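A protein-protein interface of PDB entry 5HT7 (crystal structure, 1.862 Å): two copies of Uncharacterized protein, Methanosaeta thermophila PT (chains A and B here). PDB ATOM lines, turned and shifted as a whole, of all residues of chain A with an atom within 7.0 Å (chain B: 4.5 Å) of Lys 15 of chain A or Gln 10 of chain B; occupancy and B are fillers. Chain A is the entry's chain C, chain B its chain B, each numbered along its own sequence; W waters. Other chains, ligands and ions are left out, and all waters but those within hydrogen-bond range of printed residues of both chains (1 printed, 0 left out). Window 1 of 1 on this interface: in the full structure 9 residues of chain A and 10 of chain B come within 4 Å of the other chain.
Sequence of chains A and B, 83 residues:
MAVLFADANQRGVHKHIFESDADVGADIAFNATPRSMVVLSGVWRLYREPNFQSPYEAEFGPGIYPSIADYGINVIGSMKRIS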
ATOM      1  N   ALA A   2      19.717 -27.257  21.251  1.00  0.00           N
ATOM      2  CA  ALA A   2      20.900 -28.069  21.513  1.00  0.00           C
ATOM      3  C   ALA A   2      21.097 -28.192  23.004  1.00  0.00           C
ATOM      4  O   ALA A   2      20.561 -27.389  23.771  1.00  0.00           O
ATOM      5  CB  ALA A   2      22.153 -27.461  20.861  1.00  0.00           C
ATOM      6  N   VAL A   3      21.853 -29.205  23.418  1.00  0.00           N
ATOM      7  CA  VAL A   3      22.188 -29.371  24.820  1.00  0.00           C
ATOM      8  C   VAL A   3      23.698 -29.569  24.933  1.00  0.00           C
ATOM      9  O   VAL A   3      24.283 -30.416  24.240  1.00  0.00           O
ATOM     10  CB  VAL A   3      21.447 -30.571  25.467  1.00  0.00           C
ATOM     11  CG1 VAL A   3      21.659 -30.573  26.985  1.00  0.00           C
ATOM     12  CG2 VAL A   3      19.946 -30.538  25.145  1.00  0.00           C
ATOM     13  N   LEU A   4      24.326 -28.782  25.797  1.00  0.00           N
ATOM     14  CA  LEU A   4      25.754 -28.937  26.064  1.00  0.00           C
ATOM     15  C   LEU A   4      25.941 -29.699  27.362  1.00  0.00           C
ATOM     16  O   LEU A   4      25.196 -29.474  28.314  1.00  0.00           O
ATOM     17  CB  LEU A   4      26.443 -27.570  26.155  1.00  0.00           C
ATOM     18  CG  LEU A   4      26.308 -26.623  24.961  1.00  0.00           C
ATOM     19  CD1 LEU A   4      26.963 -25.247  25.285  1.00  0.00           C
ATOM     20  CD2 LEU A   4      26.892 -27.220  23.700  1.00  0.00           C
ATOM     21  N   PHE A   5      26.956 -30.566  27.420  1.00  0.00           N
ATOM     22  CA  PHE A   5      27.244 -31.337  28.639  1.00  0.00           C
ATOM     23  C   PHE A   5      28.696 -31.133  29.083  1.00  0.00           C
ATOM     24  O   PHE A   5      29.598 -31.072  28.249  1.00  0.00           O
ATOM     25  CB  PHE A   5      26.995 -32.826  28.425  1.00  0.00           C
ATOM     26  CG  PHE A   5      25.566 -33.172  28.116  1.00  0.00           C
ATOM     27  CD1 PHE A   5      24.699 -33.542  29.124  1.00  0.00           C
ATOM     28  CD2 PHE A   5      25.108 -33.153  26.803  1.00  0.00           C
ATOM     29  CE1 PHE A   5      23.384 -33.875  28.835  1.00  0.00           C
ATOM     30  CE2 PHE A   5      23.789 -33.478  26.505  1.00  0.00           C
ATOM     31  CZ  PHE A   5      22.931 -33.838  27.527  1.00  0.00           C
ATOM     32  N   ALA A   6      28.911 -31.031  30.391  1.00  0.00           N
ATOM     33  CA  ALA A   6      30.239 -30.745  30.916  1.00  0.00           C
ATOM     34  C   ALA A   6      31.207 -31.906  30.687  1.00  0.00           C
ATOM     35  O   ALA A   6      32.403 -31.678  30.489  1.00  0.00           O
ATOM     36  CB  ALA A   6      30.167 -30.409  32.405  1.00  0.00           C
ATOM     37  N   GLY A  12      27.549 -35.046  33.298  1.00  0.00           N
ATOM     38  CA  GLY A  12      27.961 -33.828  33.964  1.00  0.00           C
ATOM     39  C   GLY A  12      26.823 -32.821  33.904  1.00  0.00           C
ATOM     40  O   GLY A  12      25.729 -33.133  33.406  1.00  0.00           O
ATOM     41  N   VAL A  13      27.063 -31.613  34.398  1.00  0.00           N
ATOM     42  CA  VAL A  13      26.018 -30.590  34.346  1.00  0.00           C
ATOM     43  C   VAL A  13      25.733 -30.284  32.885  1.00  0.00           C
ATOM     44  O   VAL A  13      26.591 -30.476  32.029  1.00  0.00           O
ATOM     45  CB  VAL A  13      26.419 -29.290  35.092  1.00  0.00           C
ATOM     46  CG1 VAL A  13      26.597 -29.576  36.576  1.00  0.00           C
ATOM     47  CG2 VAL A  13      27.690 -28.699  34.500  1.00  0.00           C
ATOM     48  N   HIS A  14      24.520 -29.830  32.587  1.00  0.00           N
ATOM     49  CA  HIS A  14      24.167 -29.572  31.197  1.00  0.00           C
ATOM     50  C   HIS A  14      23.535 -28.196  31.042  1.00  0.00           C
ATOM     51  O   HIS A  14      23.161 -27.542  32.034  1.00  0.00           O
ATOM     52  CB  HIS A  14      23.216 -30.649  30.680  1.00  0.00           C
ATOM     53  CG  HIS A  14      21.867 -30.598  31.317  1.00  0.00           C
ATOM     54  ND1 HIS A  14      21.617 -31.128  32.564  1.00  0.00           N
ATOM     55  CD2 HIS A  14      20.699 -30.059  30.893  1.00  0.00           C
ATOM     56  CE1 HIS A  14      20.356 -30.914  32.888  1.00  0.00           C
ATOM     57  NE2 HIS A  14      19.781 -30.265  31.892  1.00  0.00           N
ATOM     58  N   LYS A  15      23.426 -27.746  29.798  1.00  0.00           N
ATOM     59  CA  LYS A  15      22.895 -26.409  29.513  1.00  0.00           C
ATOM     60  C   LYS A  15      22.077 -26.456  28.231  1.00  0.00           C
ATOM     61  O   LYS A  15      22.546 -26.954  27.218  1.00  0.00           O
ATOM     62  CB  LYS A  15      24.044 -25.398  29.376  1.00  0.00           C
ATOM     63  CG  LYS A  15      23.633 -23.995  28.901  1.00  0.00           C
ATOM     64  CD  LYS A  15      24.809 -23.028  29.062  1.00  0.00           C
ATOM     65  CE  LYS A  15      24.509 -21.671  28.427  1.00  0.00           C
ATOM     66  NZ  LYS A  15      23.400 -20.968  29.098  1.00  0.00           N
ATOM     67  N   HIS A  16      20.869 -25.917  28.270  1.00  0.00           N
ATOM     68  CA  HIS A  16      20.028 -25.897  27.073  1.00  0.00           C
ATOM     69  C   HIS A  16      20.243 -24.650  26.249  1.00  0.00           C
ATOM     70  O   HIS A  16      20.210 -23.529  26.784  1.00  0.00           O
ATOM     71  CB  HIS A  16      18.557 -25.985  27.461  1.00  0.00           C
ATOM     72  CG  HIS A  16      18.222 -27.244  28.178  1.00  0.00           C
ATOM     73  ND1 HIS A  16      17.941 -28.418  27.516  1.00  0.00           N
ATOM     74  CD2 HIS A  16      18.177 -27.530  29.499  1.00  0.00           C
ATOM     75  CE1 HIS A  16      17.706 -29.371  28.401  1.00  0.00           C
ATOM     76  NE2 HIS A  16      17.857 -28.860  29.609  1.00  0.00           N
ATOM     77  N   ILE A  17      20.402 -24.836  24.945  1.00  0.00           N
ATOM     78  CA  ILE A  17      20.598 -23.706  24.033  1.00  0.00           C
ATOM     79  C   ILE A  17      19.371 -23.528  23.145  1.00  0.00           C
ATOM     80  O   ILE A  17      18.930 -24.476  22.492  1.00  0.00           O
ATOM     81  CB  ILE A  17      21.823 -23.905  23.146  1.00  0.00           C
ATOM     82  CG1 ILE A  17      23.017 -24.386  23.982  1.00  0.00           C
ATOM     83  CG2 ILE A  17      22.162 -22.623  22.368  1.00  0.00           C
ATOM     84  CD1 ILE A  17      23.499 -23.381  25.024  1.00  0.00           C
ATOM     85  N   PHE A  18      18.832 -22.313  23.124  1.00  0.00           N
ATOM     86  CA  PHE A  18      17.683 -22.013  22.271  1.00  0.00           C
ATOM     87  C   PHE A  18      18.080 -21.035  21.174  1.00  0.00           C
ATOM     88  O   PHE A  18      18.327 -19.856  21.450  1.00  0.00           O
ATOM     89  CB  PHE A  18      16.532 -21.457  23.119  1.00  0.00           C
ATOM     90  CG  PHE A  18      16.204 -22.323  24.293  1.00  0.00           C
ATOM     91  CD1 PHE A  18      15.341 -23.395  24.156  1.00  0.00           C
ATOM     92  CD2 PHE A  18      16.806 -22.102  25.520  1.00  0.00           C
ATOM     93  CE1 PHE A  18      15.061 -24.217  25.237  1.00  0.00           C
ATOM     94  CE2 PHE A  18      16.529 -22.916  26.594  1.00  0.00           C
ATOM     95  CZ  PHE A  18      15.653 -23.975  26.449  1.00  0.00           C
ATOM     96  N   SER A  20      20.454 -19.747  19.830  1.00  0.00           N
ATOM     97  CA  SER A  20      21.809 -19.200  19.910  1.00  0.00           C
ATOM     98  C   SER A  20      22.200 -18.835  21.335  1.00  0.00           C
ATOM     99  O   SER A  20      21.353 -18.666  22.212  1.00  0.00           O
ATOM    100  CB  SER A  20      21.940 -17.957  19.022  1.00  0.00           C
ATOM    101  OG  SER A  20      21.176 -16.884  19.546  1.00  0.00           O
ATOM    102  N   ASP A  21      23.502 -18.702  21.562  1.00  0.00           N
ATOM    103  CA  ASP A  21      24.000 -18.200  22.832  1.00  0.00           C
ATOM    104  C   ASP A  21      25.266 -17.432  22.540  1.00  0.00           C
ATOM    105  O   ASP A  21      26.252 -18.021  22.113  1.00  0.00           O
ATOM    106  CB  ASP A  21      24.272 -19.337  23.817  1.00  0.00           C
ATOM    107  CG  ASP A  21      24.537 -18.836  25.217  1.00  0.00           C
ATOM    108  OD1 ASP A  21      24.917 -17.650  25.395  1.00  0.00           O
ATOM    109  OD2 ASP A  21      24.352 -19.627  26.154  1.00  0.00           O
ATOM    110  N   ASP A  23      27.210 -16.051  24.628  1.00  0.00           N
ATOM    111  CA  ASP A  23      28.153 -16.056  25.747  1.00  0.00           C
ATOM    112  C   ASP A  23      27.880 -17.242  26.663  1.00  0.00           C
ATOM    113  O   ASP A  23      27.356 -17.098  27.771  1.00  0.00           O
ATOM    114  CB  ASP A  23      28.046 -14.734  26.526  1.00  0.00           C
ATOM    115  CG  ASP A  23      29.282 -14.435  27.351  1.00  0.00           C
ATOM    116  OD1 ASP A  23      30.191 -15.279  27.408  1.00  0.00           O
ATOM    117  OD2 ASP A  23      29.324 -13.342  27.952  1.00  0.00           O
ATOM    118  N   VAL A  24      28.219 -18.428  26.184  1.00  0.00           N
ATOM    119  CA  VAL A  24      27.955 -19.654  26.913  1.00  0.00           C
ATOM    120  C   VAL A  24      28.595 -19.626  28.302  1.00  0.00           C
ATOM    121  O   VAL A  24      27.986 -20.041  29.297  1.00  0.00           O
ATOM    122  CB  VAL A  24      28.470 -20.865  26.106  1.00  0.00           C
ATOM    123  CG1 VAL A  24      28.446 -22.128  26.948  1.00  0.00           C
ATOM    124  CG2 VAL A  24      27.652 -21.017  24.814  1.00  0.00           C
ATOM    125  N   GLY A  25      29.813 -19.092  28.369  1.00  0.00           N
ATOM    126  CA  GLY A  25      30.571 -19.083  29.607  1.00  0.00           C
ATOM    127  C   GLY A  25      30.020 -18.144  30.673  1.00  0.00           C
ATOM    128  O   GLY A  25      30.487 -18.147  31.808  1.00  0.00           O
ATOM    129  N   ALA A  26      29.035 -17.330  30.320  1.00  0.00           N
ATOM    130  CA  ALA A  26      28.505 -16.361  31.273  1.00  0.00           C
ATOM    131  C   ALA A  26      27.417 -16.980  32.159  1.00  0.00           C
ATOM    132  O   ALA A  26      26.886 -16.326  33.051  1.00  0.00           O
ATOM    133  CB  ALA A  26      27.958 -15.126  30.539  1.00  0.00           C
ATOM    134  N   ASP A  27      27.082 -18.240  31.907  1.00  0.00           N
ATOM    135  CA  ASP A  27      26.066 -18.936  32.694  1.00  0.00           C
ATOM    136  C   ASP A  27      26.699 -19.501  33.954  1.00  0.00           C
ATOM    137  O   ASP A  27      27.525 -20.402  33.888  1.00  0.00           O
ATOM    138  CB  ASP A  27      25.422 -20.053  31.865  1.00  0.00           C
ATOM    139  CG  ASP A  27      24.171 -20.637  32.517  1.00  0.00           C
ATOM    140  OD1 ASP A  27      24.023 -20.549  33.760  1.00  0.00           O
ATOM    141  OD2 ASP A  27      23.329 -21.184  31.769  1.00  0.00           O
ATOM    142  N   ILE A  28      26.293 -18.996  35.112  1.00  0.00           N
ATOM    143  CA  ILE A  28      26.886 -19.446  36.369  1.00  0.00           C
ATOM    144  C   ILE A  28      26.562 -20.918  36.706  1.00  0.00           C
ATOM    145  O   ILE A  28      27.254 -21.553  37.508  1.00  0.00           O
ATOM    146  CB  ILE A  28      26.433 -18.525  37.531  1.00  0.00           C
ATOM    147  CG1 ILE A  28      27.302 -18.755  38.765  1.00  0.00           C
ATOM    148  CG2 ILE A  28      24.955 -18.706  37.824  1.00  0.00           C
ATOM    149  CD1 ILE A  28      27.107 -17.729  39.846  1.00  0.00           C
ATOM    150  N   ALA A  29      25.526 -21.476  36.087  1.00  0.00           N
ATOM    151  CA  ALA A  29      25.132 -22.842  36.412  1.00  0.00           C
ATOM    152  C   ALA A  29      25.863 -23.841  35.517  1.00  0.00           C
ATOM    153  O   ALA A  29      25.746 -25.054  35.690  1.00  0.00           O
ATOM    154  CB  ALA A  29      23.646 -23.016  36.286  1.00  0.00           C
ATOM    155  N   PHE A  30      26.622 -23.318  34.565  1.00  0.00           N
ATOM    156  CA  PHE A  30      27.408 -24.150  33.670  1.00  0.00           C
ATOM    157  C   PHE A  30      28.859 -23.689  33.707  1.00  0.00           C
ATOM    158  O   PHE A  30      29.369 -23.132  32.748  1.00  0.00           O
ATOM    159  CB  PHE A  30      26.855 -24.081  32.247  1.00  0.00           C
ATOM    160  CG  PHE A  30      27.389 -25.150  31.345  1.00  0.00           C
ATOM    161  CD1 PHE A  30      26.990 -26.471  31.507  1.00  0.00           C
ATOM    162  CD2 PHE A  30      28.280 -24.837  30.333  1.00  0.00           C
ATOM    163  CE1 PHE A  30      27.478 -27.464  30.673  1.00  0.00           C
ATOM    164  CE2 PHE A  30      28.780 -25.835  29.495  1.00  0.00           C
ATOM    165  CZ  PHE A  30      28.374 -27.147  29.671  1.00  0.00           C
ATOM    166  N   PHE B   5      13.942 -20.722  34.234  1.00  0.00           N
ATOM    167  CA  PHE B   5      15.357 -20.457  34.548  1.00  0.00           C
ATOM    168  C   PHE B   5      15.489 -19.465  35.711  1.00  0.00           C
ATOM    169  O   PHE B   5      14.736 -18.498  35.800  1.00  0.00           O
ATOM    170  CB  PHE B   5      16.105 -19.902  33.325  1.00  0.00           C
ATOM    171  CG  PHE B   5      16.186 -20.858  32.181  1.00  0.00           C
ATOM    172  CD1 PHE B   5      17.291 -21.677  32.023  1.00  0.00           C
ATOM    173  CD2 PHE B   5      15.133 -20.971  31.283  1.00  0.00           C
ATOM    174  CE1 PHE B   5      17.362 -22.577  30.975  1.00  0.00           C
ATOM    175  CE2 PHE B   5      15.189 -21.876  30.229  1.00  0.00           C
ATOM    176  CZ  PHE B   5      16.300 -22.680  30.079  1.00  0.00           C
ATOM    177  N   ASP B   7      17.953 -17.408  36.334  1.00  0.00           N
ATOM    178  CA  ASP B   7      18.505 -16.136  35.892  1.00  0.00           C
ATOM    179  C   ASP B   7      17.827 -15.663  34.617  1.00  0.00           C
ATOM    180  O   ASP B   7      17.260 -16.454  33.873  1.00  0.00           O
ATOM    181  CB  ASP B   7      20.011 -16.241  35.672  1.00  0.00           C
ATOM    182  CG  ASP B   7      20.786 -16.330  36.978  1.00  0.00           C
ATOM    183  OD1 ASP B   7      20.537 -15.497  37.874  1.00  0.00           O
ATOM    184  OD2 ASP B   7      21.640 -17.228  37.106  1.00  0.00           O
ATOM    185  N   ALA B   8      17.882 -14.361  34.366  1.00  0.00           N
ATOM    186  CA  ALA B   8      17.332 -13.834  33.122  1.00  0.00           C
ATOM    187  C   ALA B   8      18.105 -14.362  31.917  1.00  0.00           C
ATOM    188  O   ALA B   8      19.231 -14.864  32.053  1.00  0.00           O
ATOM    189  CB  ALA B   8      17.342 -12.302  33.142  1.00  0.00           C
ATOM    190  N   ASN B   9      17.495 -14.260  30.737  1.00  0.00           N
ATOM    191  CA  ASN B   9      18.145 -14.664  29.497  1.00  0.00           C
ATOM    192  C   ASN B   9      18.524 -16.148  29.494  1.00  0.00           C
ATOM    193  O   ASN B   9      19.573 -16.533  28.970  1.00  0.00           O
ATOM    194  CB  ASN B   9      19.385 -13.803  29.239  1.00  0.00           C
ATOM    195  CG  ASN B   9      19.058 -12.322  29.149  1.00  0.00           C
ATOM    196  OD1 ASN B   9      19.458 -11.527  30.004  1.00  0.00           O
ATOM    197  ND2 ASN B   9      18.318 -11.947  28.119  1.00  0.00           N
ATOM    198  N   GLN B  10      17.659 -16.965  30.087  1.00  0.00           N
ATOM    199  CA  GLN B  10      17.753 -18.426  30.000  1.00  0.00           C
ATOM    200  C   GLN B  10      19.091 -18.948  30.526  1.00  0.00           C
ATOM    201  O   GLN B  10      19.754 -19.750  29.871  1.00  0.00           O
ATOM    202  CB  GLN B  10      17.554 -18.903  28.554  1.00  0.00           C
ATOM    203  CG  GLN B  10      16.217 -18.501  27.913  1.00  0.00           C
ATOM    204  CD  GLN B  10      16.120 -17.024  27.590  1.00  0.00           C
ATOM    205  OE1 GLN B  10      15.234 -16.330  28.092  1.00  0.00           O
ATOM    206  NE2 GLN B  10      17.038 -16.527  26.766  1.00  0.00           N
ATOM    207  N   ARG B  11      19.469 -18.502  31.717  1.00  0.00           N
ATOM    208  CA  ARG B  11      20.698 -18.954  32.362  1.00  0.00           C
ATOM    209  C   ARG B  11      20.386 -19.350  33.794  1.00  0.00           C
ATOM    210  O   ARG B  11      19.266 -19.158  34.267  1.00  0.00           O
ATOM    211  CB  ARG B  11      21.784 -17.857  32.315  1.00  0.00           C
ATOM    212  CG  ARG B  11      22.121 -17.398  30.891  1.00  0.00           C
ATOM    213  CD  ARG B  11      23.397 -16.549  30.805  1.00  0.00           C
ATOM    214  NE  ARG B  11      23.571 -15.959  29.470  1.00  0.00           N
ATOM    215  CZ  ARG B  11      24.122 -16.569  28.416  1.00  0.00           C
ATOM    216  NH1 ARG B  11      24.579 -17.837  28.501  1.00  0.00           N
ATOM    217  NH2 ARG B  11      24.216 -15.899  27.258  1.00  0.00           N
ATOM    218  N   SER B  36      13.405 -16.112  33.865  1.00  0.00           N
ATOM    219  CA  SER B  36      13.120 -16.261  32.447  1.00  0.00           C
ATOM    220  C   SER B  36      12.470 -17.622  32.195  1.00  0.00           C
ATOM    221  O   SER B  36      12.470 -18.489  33.077  1.00  0.00           O
ATOM    222  CB  SER B  36      14.384 -16.082  31.595  1.00  0.00           C
ATOM    223  OG  SER B  36      15.394 -17.029  31.914  1.00  0.00           O
ATOM    224  N   VAL B  38      11.179 -20.501  28.807  1.00  0.00           N
ATOM    225  CA  VAL B  38      10.972 -20.868  27.425  1.00  0.00           C
ATOM    226  C   VAL B  38       9.751 -21.774  27.378  1.00  0.00           C
ATOM    227  O   VAL B  38       9.650 -22.713  28.154  1.00  0.00           O
ATOM    228  CB  VAL B  38      12.205 -21.587  26.831  1.00  0.00           C
ATOM    229  CG1 VAL B  38      11.939 -22.026  25.390  1.00  0.00           C
ATOM    230  CG2 VAL B  38      13.416 -20.689  26.905  1.00  0.00           C
ATOM    231  N   ILE B  64      10.447 -17.502  23.686  1.00  0.00           N
ATOM    232  CA  ILE B  64      11.513 -17.261  24.637  1.00  0.00           C
ATOM    233  C   ILE B  64      11.217 -15.975  25.378  1.00  0.00           C
ATOM    234  O   ILE B  64      10.998 -14.943  24.750  1.00  0.00           O
ATOM    235  CB  ILE B  64      12.867 -17.160  23.917  1.00  0.00           C
ATOM    236  CG1 ILE B  64      13.119 -18.447  23.126  1.00  0.00           C
ATOM    237  CG2 ILE B  64      13.979 -16.850  24.917  1.00  0.00           C
ATOM    238  CD1 ILE B  64      14.312 -18.369  22.178  1.00  0.00           C
ATOM    239  N   TYR B  65      11.197 -16.039  26.707  1.00  0.00           N
ATOM    240  CA  TYR B  65      10.830 -14.894  27.544  1.00  0.00           C
ATOM    241  C   TYR B  65      11.973 -14.558  28.496  1.00  0.00           C
ATOM    242  O   TYR B  65      12.028 -15.082  29.609  1.00  0.00           O
ATOM    243  CB  TYR B  65       9.542 -15.207  28.320  1.00  0.00           C
ATOM    244  CG  TYR B  65       8.420 -15.607  27.384  1.00  0.00           C
ATOM    245  CD1 TYR B  65       7.649 -14.640  26.748  1.00  0.00           C
ATOM    246  CD2 TYR B  65       8.169 -16.940  27.090  1.00  0.00           C
ATOM    247  CE1 TYR B  65       6.633 -14.994  25.856  1.00  0.00           C
ATOM    248  CE2 TYR B  65       7.148 -17.302  26.202  1.00  0.00           C
ATOM    249  CZ  TYR B  65       6.385 -16.313  25.591  1.00  0.00           C
ATOM    250  OH  TYR B  65       5.370 -16.654  24.704  1.00  0.00           O
ATOM    251  N   PRO B  66      12.899 -13.690  28.055  1.00  0.00           N
ATOM    252  CA  PRO B  66      14.191 -13.512  28.740  1.00  0.00           C
ATOM    253  C   PRO B  66      14.109 -12.796  30.074  1.00  0.00           C
ATOM    254  O   PRO B  66      15.070 -12.842  30.851  1.00  0.00           O
ATOM    255  CB  PRO B  66      15.014 -12.685  27.733  1.00  0.00           C
ATOM    256  CG  PRO B  66      14.016 -12.014  26.882  1.00  0.00           C
ATOM    257  CD  PRO B  66      12.831 -12.941  26.790  1.00  0.00           C
HETATM  258  O   HOH W   1      20.731 -22.019  28.894  1.00  0.00           O
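The side-chain carboxylate (OD1) of Asp 21 of chain A is in salt-bridge range of the guanidinium group (NH2) of Arg 11 of chain B.
NZ of Lys 15 of chain A lies close to NH1 of Arg 11 of chain B (3.4 Å).
NH1 of Arg 11 of chain B lies within hydrogen-bond range of O of Asp 23 of chain A.
O of Gln 10 of chain B touches NZ of Lys 15 of chain A, 3.9 Å away.
Phe 5 of chain B touches Phe 18 of chain A.
Phe 18 of chain A touches Val 38 of chain B (CE1 to CG1, 3.8 Å).
CB of Phe 18 of chain A touches CD1 of Ile 64 of chain B, at 3.9 Å.
Asp 27 of chain A touches Arg 11 of chain B.
Asp 7 of chain B touches Ile 28 of chain A (OD2 to CG2, 3.7 Å).
Lys 15 of chain A touches just these residues of chain B: Gln 10 (3.9 Å) and Arg 11 (3.4 Å).
Gln 10 of chain B touches just one residue of chain A: Lys 15.
Printed residues of chain A within 4 Å of Asp 7 of chain B: Ile 28 (3.7 Å).
Of the printed residues of chain A, Arg 11 of chain B touches Lys 15, Asp 21, Asp 23 and Asp 27.
Printed residues of chain B within 4 Å of Asp 27 of chain A: Arg 11 (3.5 Å).
Of the printed residues of chain A, Phe 5 of chain B touches Phe 18 (3.5 Å).
Printed residues of chain A within 4 Å of Val 38 of chain B: Phe 18 (3.8 Å).
1 position is printed for both chains.
Of the 9 pairs that touch across the chains among the printed residues, none has its exchanged pair printed and touching as well.
Of the 22 printed residues of chain A, 6 touch a printed residue of chain B.
Printed residues of chain A that touch a printed residue of chain B: Lys 15, Phe 18, Asp 21, Asp 23, Asp 27 and Ile 28.
Hydrophobic or aromatic side chains of chain A that line the printed part of chain B: Phe 18 and Ile 28.
Along chain A the printed residues that touch a printed residue of chain B span positions 15 to 28.
Hydrophobic or aromatic side chains of chain B within 4 Å of the printed part of chain A: Phe 5, Val 38 and Ile 64.
Among the printed residues, Asp or Glu carboxylates within 4 Å of a Lys or Arg side-chain nitrogen of the other chain: Asp 21 of chain A with Arg 11 of chain B (2.7 Å).
Water W1 lies within hydrogen-bond range of the backbone carbonyl oxygen (O) of His 16 of chain A, the backbone carbonyl oxygen (O) of Gln 10 of chain B and the side-chain amino group (NZ) of Lys 15 of chain A.
O of Ser 36 of chain B sits at hydrogen-bond distance from N of Phe 5 of chain B.
OD1 of Asp 21 of chain A lies within hydrogen-bond range of N of Asp 23 of chain A (2.9 Å).
The side-chain amino group (NZ) of Lys 15 of chain A is in salt-bridge range of the side-chain carboxylate (OD2) of Asp 21 of chain A (3.4 Å).
O of Leu 4 of chain A lies within hydrogen-bond range of N of Lys 15 of chain A, at 2.9 Å.
The side-chain carboxylate (OD2) of Asp 27 of chain A is in salt-bridge range of the side-chain amino group (NZ) of Lys 15 of chain A, at 2.7 Å.
The side-chain carboxylate (OD1) of Asp 21 of chain A sits at hydrogen-bond distance from the backbone NH (N) of Val 24 of chain A (3.5 Å).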
